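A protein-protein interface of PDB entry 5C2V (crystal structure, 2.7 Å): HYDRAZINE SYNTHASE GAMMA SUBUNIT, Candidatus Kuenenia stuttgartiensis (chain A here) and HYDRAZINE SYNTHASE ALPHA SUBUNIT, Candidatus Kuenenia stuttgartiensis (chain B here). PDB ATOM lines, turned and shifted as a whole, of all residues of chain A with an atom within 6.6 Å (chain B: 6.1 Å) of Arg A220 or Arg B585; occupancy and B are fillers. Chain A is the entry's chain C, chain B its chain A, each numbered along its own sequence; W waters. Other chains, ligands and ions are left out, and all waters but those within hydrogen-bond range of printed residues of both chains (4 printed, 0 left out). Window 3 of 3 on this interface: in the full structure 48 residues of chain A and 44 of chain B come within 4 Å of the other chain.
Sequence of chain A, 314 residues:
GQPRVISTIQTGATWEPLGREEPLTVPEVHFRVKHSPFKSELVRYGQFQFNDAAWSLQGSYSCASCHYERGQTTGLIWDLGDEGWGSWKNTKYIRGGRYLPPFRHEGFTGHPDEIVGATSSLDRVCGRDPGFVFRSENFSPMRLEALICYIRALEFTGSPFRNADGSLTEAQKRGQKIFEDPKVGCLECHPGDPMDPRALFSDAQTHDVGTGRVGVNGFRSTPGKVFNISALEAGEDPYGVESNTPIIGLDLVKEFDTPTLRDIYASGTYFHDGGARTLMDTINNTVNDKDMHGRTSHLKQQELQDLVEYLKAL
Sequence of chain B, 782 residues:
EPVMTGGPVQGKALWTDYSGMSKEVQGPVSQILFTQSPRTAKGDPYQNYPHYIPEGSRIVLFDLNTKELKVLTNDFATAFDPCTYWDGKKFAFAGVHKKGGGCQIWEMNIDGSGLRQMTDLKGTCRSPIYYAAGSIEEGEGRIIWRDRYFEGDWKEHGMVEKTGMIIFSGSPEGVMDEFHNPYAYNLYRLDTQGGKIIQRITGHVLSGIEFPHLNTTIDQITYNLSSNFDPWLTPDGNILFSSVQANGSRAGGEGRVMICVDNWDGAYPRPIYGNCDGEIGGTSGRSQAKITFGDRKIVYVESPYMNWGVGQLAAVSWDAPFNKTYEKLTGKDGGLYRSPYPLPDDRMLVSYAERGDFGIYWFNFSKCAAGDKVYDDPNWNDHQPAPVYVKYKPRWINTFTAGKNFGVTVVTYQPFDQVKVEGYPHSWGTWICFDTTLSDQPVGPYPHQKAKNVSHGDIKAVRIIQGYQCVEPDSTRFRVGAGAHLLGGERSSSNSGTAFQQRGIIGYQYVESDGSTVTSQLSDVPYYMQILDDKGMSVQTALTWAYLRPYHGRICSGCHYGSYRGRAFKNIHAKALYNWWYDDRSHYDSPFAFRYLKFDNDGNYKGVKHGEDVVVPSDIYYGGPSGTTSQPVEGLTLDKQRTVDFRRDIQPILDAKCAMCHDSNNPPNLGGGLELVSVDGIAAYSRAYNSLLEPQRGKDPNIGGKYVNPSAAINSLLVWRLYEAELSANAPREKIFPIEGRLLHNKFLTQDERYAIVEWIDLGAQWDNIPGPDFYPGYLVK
OD1 of Asp B583 is in salt-bridge range of NE of Arg A220 (3.5 Å). The guanidinium group of Arg A220 sits close to the guanidinium group of Arg B585 (3.3 Å).
NE1 of Trp B581 is in hydrogen-bond range of O of Asp B583 (2.7 Å). The guanidinium group of Arg B585 is in salt-bridge range of the side-chain carboxylate of Asp B583 (3.0 Å).
Among the printed residues, merely in contact across the chains: Leu A252 with Tyr B582 (3.3 Å), Thr A222 with Tyr B582 (3.5 Å), Arg A220 with Tyr B582 (3.7 Å), Leu A250 with Tyr B582 (3.7 Å), Leu A252 with Asp B584 (3.9 Å) and Arg A220 with Asp B584 (3.98 Å).
Arg A220 touches just these residues of chain B: Tyr B582, Asp B583, Asp B584 and Arg B585. Asp A251 touches none of the printed residues of chain B. Of the printed residues of chain B, Leu A252 touches Tyr B582 and Asp B584. Trp B581 touches none of the printed residues of chain A. Of the printed residues of chain A, Tyr B582 touches Arg A220, Thr A222, Leu A250 and Leu A252. Printed residues of chain A within 4 Å of Asp B583: Arg A220. Printed residues of chain A within 4 Å of Asp B584: Arg A220 (3.98 Å) and Leu A252 (3.9 Å). Arg B585 touches just one residue of chain A: Arg A220. The nearest printed residue of chain B that does not touch Arg A220 is Ser B586 (7.5 Å).
Of the 11 printed residues of chain A, 4 touch a printed residue of chain B. Of the 10 printed residues of chain B, 4 touch a printed residue of chain A. Among the printed residues, 8 pairs touch across the chains. Among the printed residues, Asp or Glu carboxylates within 4 Å of a Lys or Arg side-chain nitrogen of the other chain: Arg A220 with Asp B583 (3.5 Å).
Water W3 bridges the backbone carbonyl oxygen of Arg A220 and the side-chain carboxylate of Asp B583. Water W1 lies within hydrogen-bond range of the backbone carbonyl oxygen (O) of Leu A252, the backbone NH (N) of Asp B584 and the guanidinium group (NE) of Arg A220. Water W2 lies within hydrogen-bond range of O of Ser A221 (2.9 Å) and O of Tyr B582 (3.2 Å). Water W4 lies within hydrogen-bond range of the backbone carbonyl oxygen (O) of Leu A250 and the backbone carbonyl oxygen (O) of Trp B581.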
ATOM      1  N   ARG A 213      11.570   8.510 -28.802  1.00  0.00           N
ATOM      2  CA  ARG A 213      12.904   8.022 -28.469  1.00  0.00           C
ATOM      3  C   ARG A 213      13.535   8.895 -27.389  1.00  0.00           C
ATOM      4  O   ARG A 213      13.714  10.097 -27.581  1.00  0.00           O
ATOM      5  CB  ARG A 213      13.796   7.992 -29.712  1.00  0.00           C
ATOM      6  CG  ARG A 213      13.151   7.352 -30.935  1.00  0.00           C
ATOM      7  CD  ARG A 213      12.578   5.982 -30.619  1.00  0.00           C
ATOM      8  NE  ARG A 213      11.918   5.390 -31.780  1.00  0.00           N
ATOM      9  CZ  ARG A 213      11.111   4.336 -31.723  1.00  0.00           C
ATOM     10  NH1 ARG A 213      10.858   3.754 -30.558  1.00  0.00           N
ATOM     11  NH2 ARG A 213      10.555   3.863 -32.830  1.00  0.00           N
ATOM     12  N   VAL A 214      13.871   8.286 -26.258  1.00  0.00           N
ATOM     13  CA  VAL A 214      14.419   9.033 -25.132  1.00  0.00           C
ATOM     14  C   VAL A 214      15.808   8.543 -24.736  1.00  0.00           C
ATOM     15  O   VAL A 214      16.336   7.596 -25.319  1.00  0.00           O
ATOM     16  CB  VAL A 214      13.495   8.949 -23.903  1.00  0.00           C
ATOM     17  CG1 VAL A 214      12.167   9.631 -24.191  1.00  0.00           C
ATOM     18  CG2 VAL A 214      13.281   7.499 -23.499  1.00  0.00           C
ATOM     19  N   GLY A 215      16.390   9.197 -23.735  1.00  0.00           N
ATOM     20  CA  GLY A 215      17.718   8.853 -23.267  1.00  0.00           C
ATOM     21  C   GLY A 215      17.703   7.811 -22.168  1.00  0.00           C
ATOM     22  O   GLY A 215      16.639   7.370 -21.733  1.00  0.00           O
ATOM     23  N   GLY A 218      16.037   9.118 -19.294  1.00  0.00           N
ATOM     24  CA  GLY A 218      14.698   9.587 -19.602  1.00  0.00           C
ATOM     25  C   GLY A 218      14.665  10.740 -20.587  1.00  0.00           C
ATOM     26  O   GLY A 218      15.668  11.040 -21.235  1.00  0.00           O
ATOM     27  N   PHE A 219      13.500  11.369 -20.713  1.00  0.00           N
ATOM     28  CA  PHE A 219      13.297  12.470 -21.652  1.00  0.00           C
ATOM     29  C   PHE A 219      14.304  13.598 -21.428  1.00  0.00           C
ATOM     30  O   PHE A 219      14.639  13.922 -20.288  1.00  0.00           O
ATOM     31  CB  PHE A 219      11.866  13.005 -21.532  1.00  0.00           C
ATOM     32  CG  PHE A 219      11.484  13.987 -22.606  1.00  0.00           C
ATOM     33  CD1 PHE A 219      11.468  13.607 -23.939  1.00  0.00           C
ATOM     34  CD2 PHE A 219      11.120  15.283 -22.280  1.00  0.00           C
ATOM     35  CE1 PHE A 219      11.110  14.507 -24.927  1.00  0.00           C
ATOM     36  CE2 PHE A 219      10.761  16.187 -23.263  1.00  0.00           C
ATOM     37  CZ  PHE A 219      10.757  15.798 -24.587  1.00  0.00           C
ATOM     38  N   ARG A 220      14.787  14.171 -22.529  1.00  0.00           N
ATOM     39  CA  ARG A 220      15.758  15.268 -22.509  1.00  0.00           C
ATOM     40  C   ARG A 220      17.081  14.896 -21.842  1.00  0.00           C
ATOM     41  O   ARG A 220      17.763  15.758 -21.285  1.00  0.00           O
ATOM     42  CB  ARG A 220      15.162  16.498 -21.816  1.00  0.00           C
ATOM     43  CG  ARG A 220      14.086  17.204 -22.619  1.00  0.00           C
ATOM     44  CD  ARG A 220      13.333  18.210 -21.767  1.00  0.00           C
ATOM     45  NE  ARG A 220      12.372  18.979 -22.551  1.00  0.00           N
ATOM     46  CZ  ARG A 220      11.452  19.783 -22.029  1.00  0.00           C
ATOM     47  NH1 ARG A 220      11.360  19.923 -20.713  1.00  0.00           N
ATOM     48  NH2 ARG A 220      10.621  20.445 -22.822  1.00  0.00           N
ATOM     49  N   SER A 221      17.447  13.620 -21.900  1.00  0.00           N
ATOM     50  CA  SER A 221      18.732  13.181 -21.365  1.00  0.00           C
ATOM     51  C   SER A 221      19.612  12.588 -22.463  1.00  0.00           C
ATOM     52  O   SER A 221      19.190  12.474 -23.613  1.00  0.00           O
ATOM     53  CB  SER A 221      18.530  12.161 -20.245  1.00  0.00           C
ATOM     54  OG  SER A 221      17.992  10.950 -20.747  1.00  0.00           O
ATOM     55  N   THR A 222      20.834  12.213 -22.099  1.00  0.00           N
ATOM     56  CA  THR A 222      21.790  11.659 -23.053  1.00  0.00           C
ATOM     57  C   THR A 222      22.683  10.633 -22.351  1.00  0.00           C
ATOM     58  O   THR A 222      22.961  10.768 -21.157  1.00  0.00           O
ATOM     59  CB  THR A 222      22.641  12.786 -23.697  1.00  0.00           C
ATOM     60  OG1 THR A 222      23.436  12.259 -24.766  1.00  0.00           O
ATOM     61  CG2 THR A 222      23.543  13.449 -22.666  1.00  0.00           C
ATOM     62  N   LEU A 250      17.412  10.359 -29.832  1.00  0.00           N
ATOM     63  CA  LEU A 250      16.922  11.291 -28.827  1.00  0.00           C
ATOM     64  C   LEU A 250      15.913  12.243 -29.452  1.00  0.00           C
ATOM     65  O   LEU A 250      16.278  13.102 -30.246  1.00  0.00           O
ATOM     66  CB  LEU A 250      18.076  12.083 -28.210  1.00  0.00           C
ATOM     67  CG  LEU A 250      19.123  11.290 -27.431  1.00  0.00           C
ATOM     68  CD1 LEU A 250      20.304  12.172 -27.053  1.00  0.00           C
ATOM     69  CD2 LEU A 250      18.483  10.693 -26.198  1.00  0.00           C
ATOM     70  N   ASP A 251      14.647  12.107 -29.067  1.00  0.00           N
ATOM     71  CA  ASP A 251      13.587  12.936 -29.629  1.00  0.00           C
ATOM     72  C   ASP A 251      13.297  14.146 -28.750  1.00  0.00           C
ATOM     73  O   ASP A 251      13.377  14.072 -27.524  1.00  0.00           O
ATOM     74  CB  ASP A 251      12.309  12.119 -29.827  1.00  0.00           C
ATOM     75  CG  ASP A 251      12.400  11.163 -31.002  1.00  0.00           C
ATOM     76  OD1 ASP A 251      13.251  11.381 -31.888  1.00  0.00           O
ATOM     77  OD2 ASP A 251      11.608  10.195 -31.039  1.00  0.00           O
ATOM     78  N   LEU A 252      12.969  15.266 -29.385  1.00  0.00           N
ATOM     79  CA  LEU A 252      12.614  16.472 -28.647  1.00  0.00           C
ATOM     80  C   LEU A 252      11.143  16.456 -28.233  1.00  0.00           C
ATOM     81  O   LEU A 252      10.722  17.246 -27.388  1.00  0.00           O
ATOM     82  CB  LEU A 252      12.918  17.721 -29.477  1.00  0.00           C
ATOM     83  CG  LEU A 252      14.247  18.421 -29.172  1.00  0.00           C
ATOM     84  CD1 LEU A 252      15.427  17.475 -29.344  1.00  0.00           C
ATOM     85  CD2 LEU A 252      14.414  19.667 -30.032  1.00  0.00           C
ATOM     86  N   TRP B 581      22.918  18.569 -29.405  1.00  0.00           N
ATOM     87  CA  TRP B 581      21.676  19.223 -28.995  1.00  0.00           C
ATOM     88  C   TRP B 581      20.545  18.205 -28.817  1.00  0.00           C
ATOM     89  O   TRP B 581      19.946  17.762 -29.798  1.00  0.00           O
ATOM     90  CB  TRP B 581      21.315  20.277 -30.052  1.00  0.00           C
ATOM     91  CG  TRP B 581      19.995  20.974 -29.906  1.00  0.00           C
ATOM     92  CD1 TRP B 581      19.306  21.212 -28.754  1.00  0.00           C
ATOM     93  CD2 TRP B 581      19.211  21.538 -30.967  1.00  0.00           C
ATOM     94  NE1 TRP B 581      18.138  21.886 -29.032  1.00  0.00           N
ATOM     95  CE2 TRP B 581      18.058  22.097 -30.384  1.00  0.00           C
ATOM     96  CE3 TRP B 581      19.375  21.624 -32.353  1.00  0.00           C
ATOM     97  CZ2 TRP B 581      17.072  22.729 -31.140  1.00  0.00           C
ATOM     98  CZ3 TRP B 581      18.394  22.249 -33.101  1.00  0.00           C
ATOM     99  CH2 TRP B 581      17.259  22.795 -32.492  1.00  0.00           C
ATOM    100  N   TYR B 582      20.244  17.843 -27.570  1.00  0.00           N
ATOM    101  CA  TYR B 582      19.110  16.961 -27.278  1.00  0.00           C
ATOM    102  C   TYR B 582      17.887  17.595 -26.597  1.00  0.00           C
ATOM    103  O   TYR B 582      16.885  16.912 -26.387  1.00  0.00           O
ATOM    104  CB  TYR B 582      19.583  15.763 -26.444  1.00  0.00           C
ATOM    105  CG  TYR B 582      20.537  16.096 -25.323  1.00  0.00           C
ATOM    106  CD1 TYR B 582      20.070  16.375 -24.046  1.00  0.00           C
ATOM    107  CD2 TYR B 582      21.909  16.109 -25.537  1.00  0.00           C
ATOM    108  CE1 TYR B 582      20.943  16.671 -23.017  1.00  0.00           C
ATOM    109  CE2 TYR B 582      22.788  16.404 -24.518  1.00  0.00           C
ATOM    110  CZ  TYR B 582      22.301  16.685 -23.259  1.00  0.00           C
ATOM    111  OH  TYR B 582      23.177  16.979 -22.240  1.00  0.00           O
ATOM    112  N   ASP B 583      17.953  18.876 -26.244  1.00  0.00           N
ATOM    113  CA  ASP B 583      16.896  19.465 -25.414  1.00  0.00           C
ATOM    114  C   ASP B 583      16.102  20.543 -26.149  1.00  0.00           C
ATOM    115  O   ASP B 583      16.665  21.367 -26.870  1.00  0.00           O
ATOM    116  CB  ASP B 583      17.492  20.041 -24.124  1.00  0.00           C
ATOM    117  CG  ASP B 583      16.456  20.233 -23.025  1.00  0.00           C
ATOM    118  OD1 ASP B 583      15.307  20.617 -23.332  1.00  0.00           O
ATOM    119  OD2 ASP B 583      16.794  20.000 -21.845  1.00  0.00           O
ATOM    120  N   ASP B 584      14.787  20.529 -25.945  1.00  0.00           N
ATOM    121  CA  ASP B 584      13.871  21.450 -26.612  1.00  0.00           C
ATOM    122  C   ASP B 584      14.104  22.900 -26.193  1.00  0.00           C
ATOM    123  O   ASP B 584      13.917  23.825 -26.984  1.00  0.00           O
ATOM    124  CB  ASP B 584      12.420  21.056 -26.314  1.00  0.00           C
ATOM    125  CG  ASP B 584      11.444  21.574 -27.355  1.00  0.00           C
ATOM    126  OD1 ASP B 584      11.853  22.382 -28.213  1.00  0.00           O
ATOM    127  OD2 ASP B 584      10.262  21.172 -27.311  1.00  0.00           O
ATOM    128  N   ARG B 585      14.520  23.087 -24.947  1.00  0.00           N
ATOM    129  CA  ARG B 585      14.635  24.418 -24.361  1.00  0.00           C
ATOM    130  C   ARG B 585      16.006  25.048 -24.591  1.00  0.00           C
ATOM    131  O   ARG B 585      16.284  26.137 -24.089  1.00  0.00           O
ATOM    132  CB  ARG B 585      14.343  24.351 -22.860  1.00  0.00           C
ATOM    133  CG  ARG B 585      12.965  23.801 -22.521  1.00  0.00           C
ATOM    134  CD  ARG B 585      12.909  23.281 -21.092  1.00  0.00           C
ATOM    135  NE  ARG B 585      13.792  22.135 -20.894  1.00  0.00           N
ATOM    136  CZ  ARG B 585      13.939  21.492 -19.739  1.00  0.00           C
ATOM    137  NH1 ARG B 585      13.258  21.880 -18.670  1.00  0.00           N
ATOM    138  NH2 ARG B 585      14.765  20.458 -19.655  1.00  0.00           N
ATOM    139  N   SER B 586      16.860  24.365 -25.348  1.00  0.00           N
ATOM    140  CA  SER B 586      18.243  24.803 -25.509  1.00  0.00           C
ATOM    141  C   SER B 586      18.632  25.123 -26.951  1.00  0.00           C
ATOM    142  O   SER B 586      18.067  24.572 -27.896  1.00  0.00           O
ATOM    143  CB  SER B 586      19.192  23.735 -24.961  1.00  0.00           C
ATOM    144  OG  SER B 586      18.897  23.432 -23.610  1.00  0.00           O
ATOM    145  N   HIS B 587      19.597  26.028 -27.107  1.00  0.00           N
ATOM    146  CA  HIS B 587      20.267  26.228 -28.388  1.00  0.00           C
ATOM    147  C   HIS B 587      21.254  25.088 -28.620  1.00  0.00           C
ATOM    148  O   HIS B 587      21.272  24.467 -29.684  1.00  0.00           O
ATOM    149  CB  HIS B 587      20.999  27.572 -28.429  1.00  0.00           C
ATOM    150  CG  HIS B 587      20.095  28.763 -28.341  1.00  0.00           C
ATOM    151  ND1 HIS B 587      19.028  28.954 -29.191  1.00  0.00           N
ATOM    152  CD2 HIS B 587      20.111  29.834 -27.511  1.00  0.00           C
ATOM    153  CE1 HIS B 587      18.420  30.086 -28.883  1.00  0.00           C
ATOM    154  NE2 HIS B 587      19.058  30.639 -27.868  1.00  0.00           N
ATOM    155  N   GLY B 627      18.684  30.254 -19.321  1.00  0.00           N
ATOM    156  CA  GLY B 627      18.404  28.831 -19.369  1.00  0.00           C
ATOM    157  C   GLY B 627      18.278  28.314 -20.787  1.00  0.00           C
ATOM    158  O   GLY B 627      17.437  27.461 -21.076  1.00  0.00           O
ATOM    159  N   THR B 628      19.115  28.835 -21.679  1.00  0.00           N
ATOM    160  CA  THR B 628      19.108  28.414 -23.076  1.00  0.00           C
ATOM    161  C   THR B 628      20.124  27.301 -23.329  1.00  0.00           C
ATOM    162  O   THR B 628      20.342  26.899 -24.471  1.00  0.00           O
ATOM    163  CB  THR B 628      19.392  29.593 -24.022  1.00  0.00           C
ATOM    164  OG1 THR B 628      20.594  30.256 -23.617  1.00  0.00           O
ATOM    165  CG2 THR B 628      18.236  30.582 -23.994  1.00  0.00           C
ATOM    166  N   THR B 629      20.762  26.827 -22.263  1.00  0.00           N
ATOM    167  CA  THR B 629      21.626  25.653 -22.350  1.00  0.00           C
ATOM    168  C   THR B 629      21.536  24.834 -21.065  1.00  0.00           C
ATOM    169  O   THR B 629      21.360  25.383 -19.976  1.00  0.00           O
ATOM    170  CB  THR B 629      23.097  26.037 -22.628  1.00  0.00           C
ATOM    171  OG1 THR B 629      23.890  24.849 -22.739  1.00  0.00           O
ATOM    172  CG2 THR B 629      23.653  26.913 -21.514  1.00  0.00           C
HETATM  173  O   HOH W   1      12.825  17.910 -25.758  1.00  0.00           O
HETATM  174  O   HOH W   2      17.259  13.927 -25.168  1.00  0.00           O
HETATM  175  O   HOH W   3      18.303  18.154 -20.684  1.00  0.00           O
HETATM  176  O   HOH W   4      17.952  15.457 -30.075  1.00  0.00           O
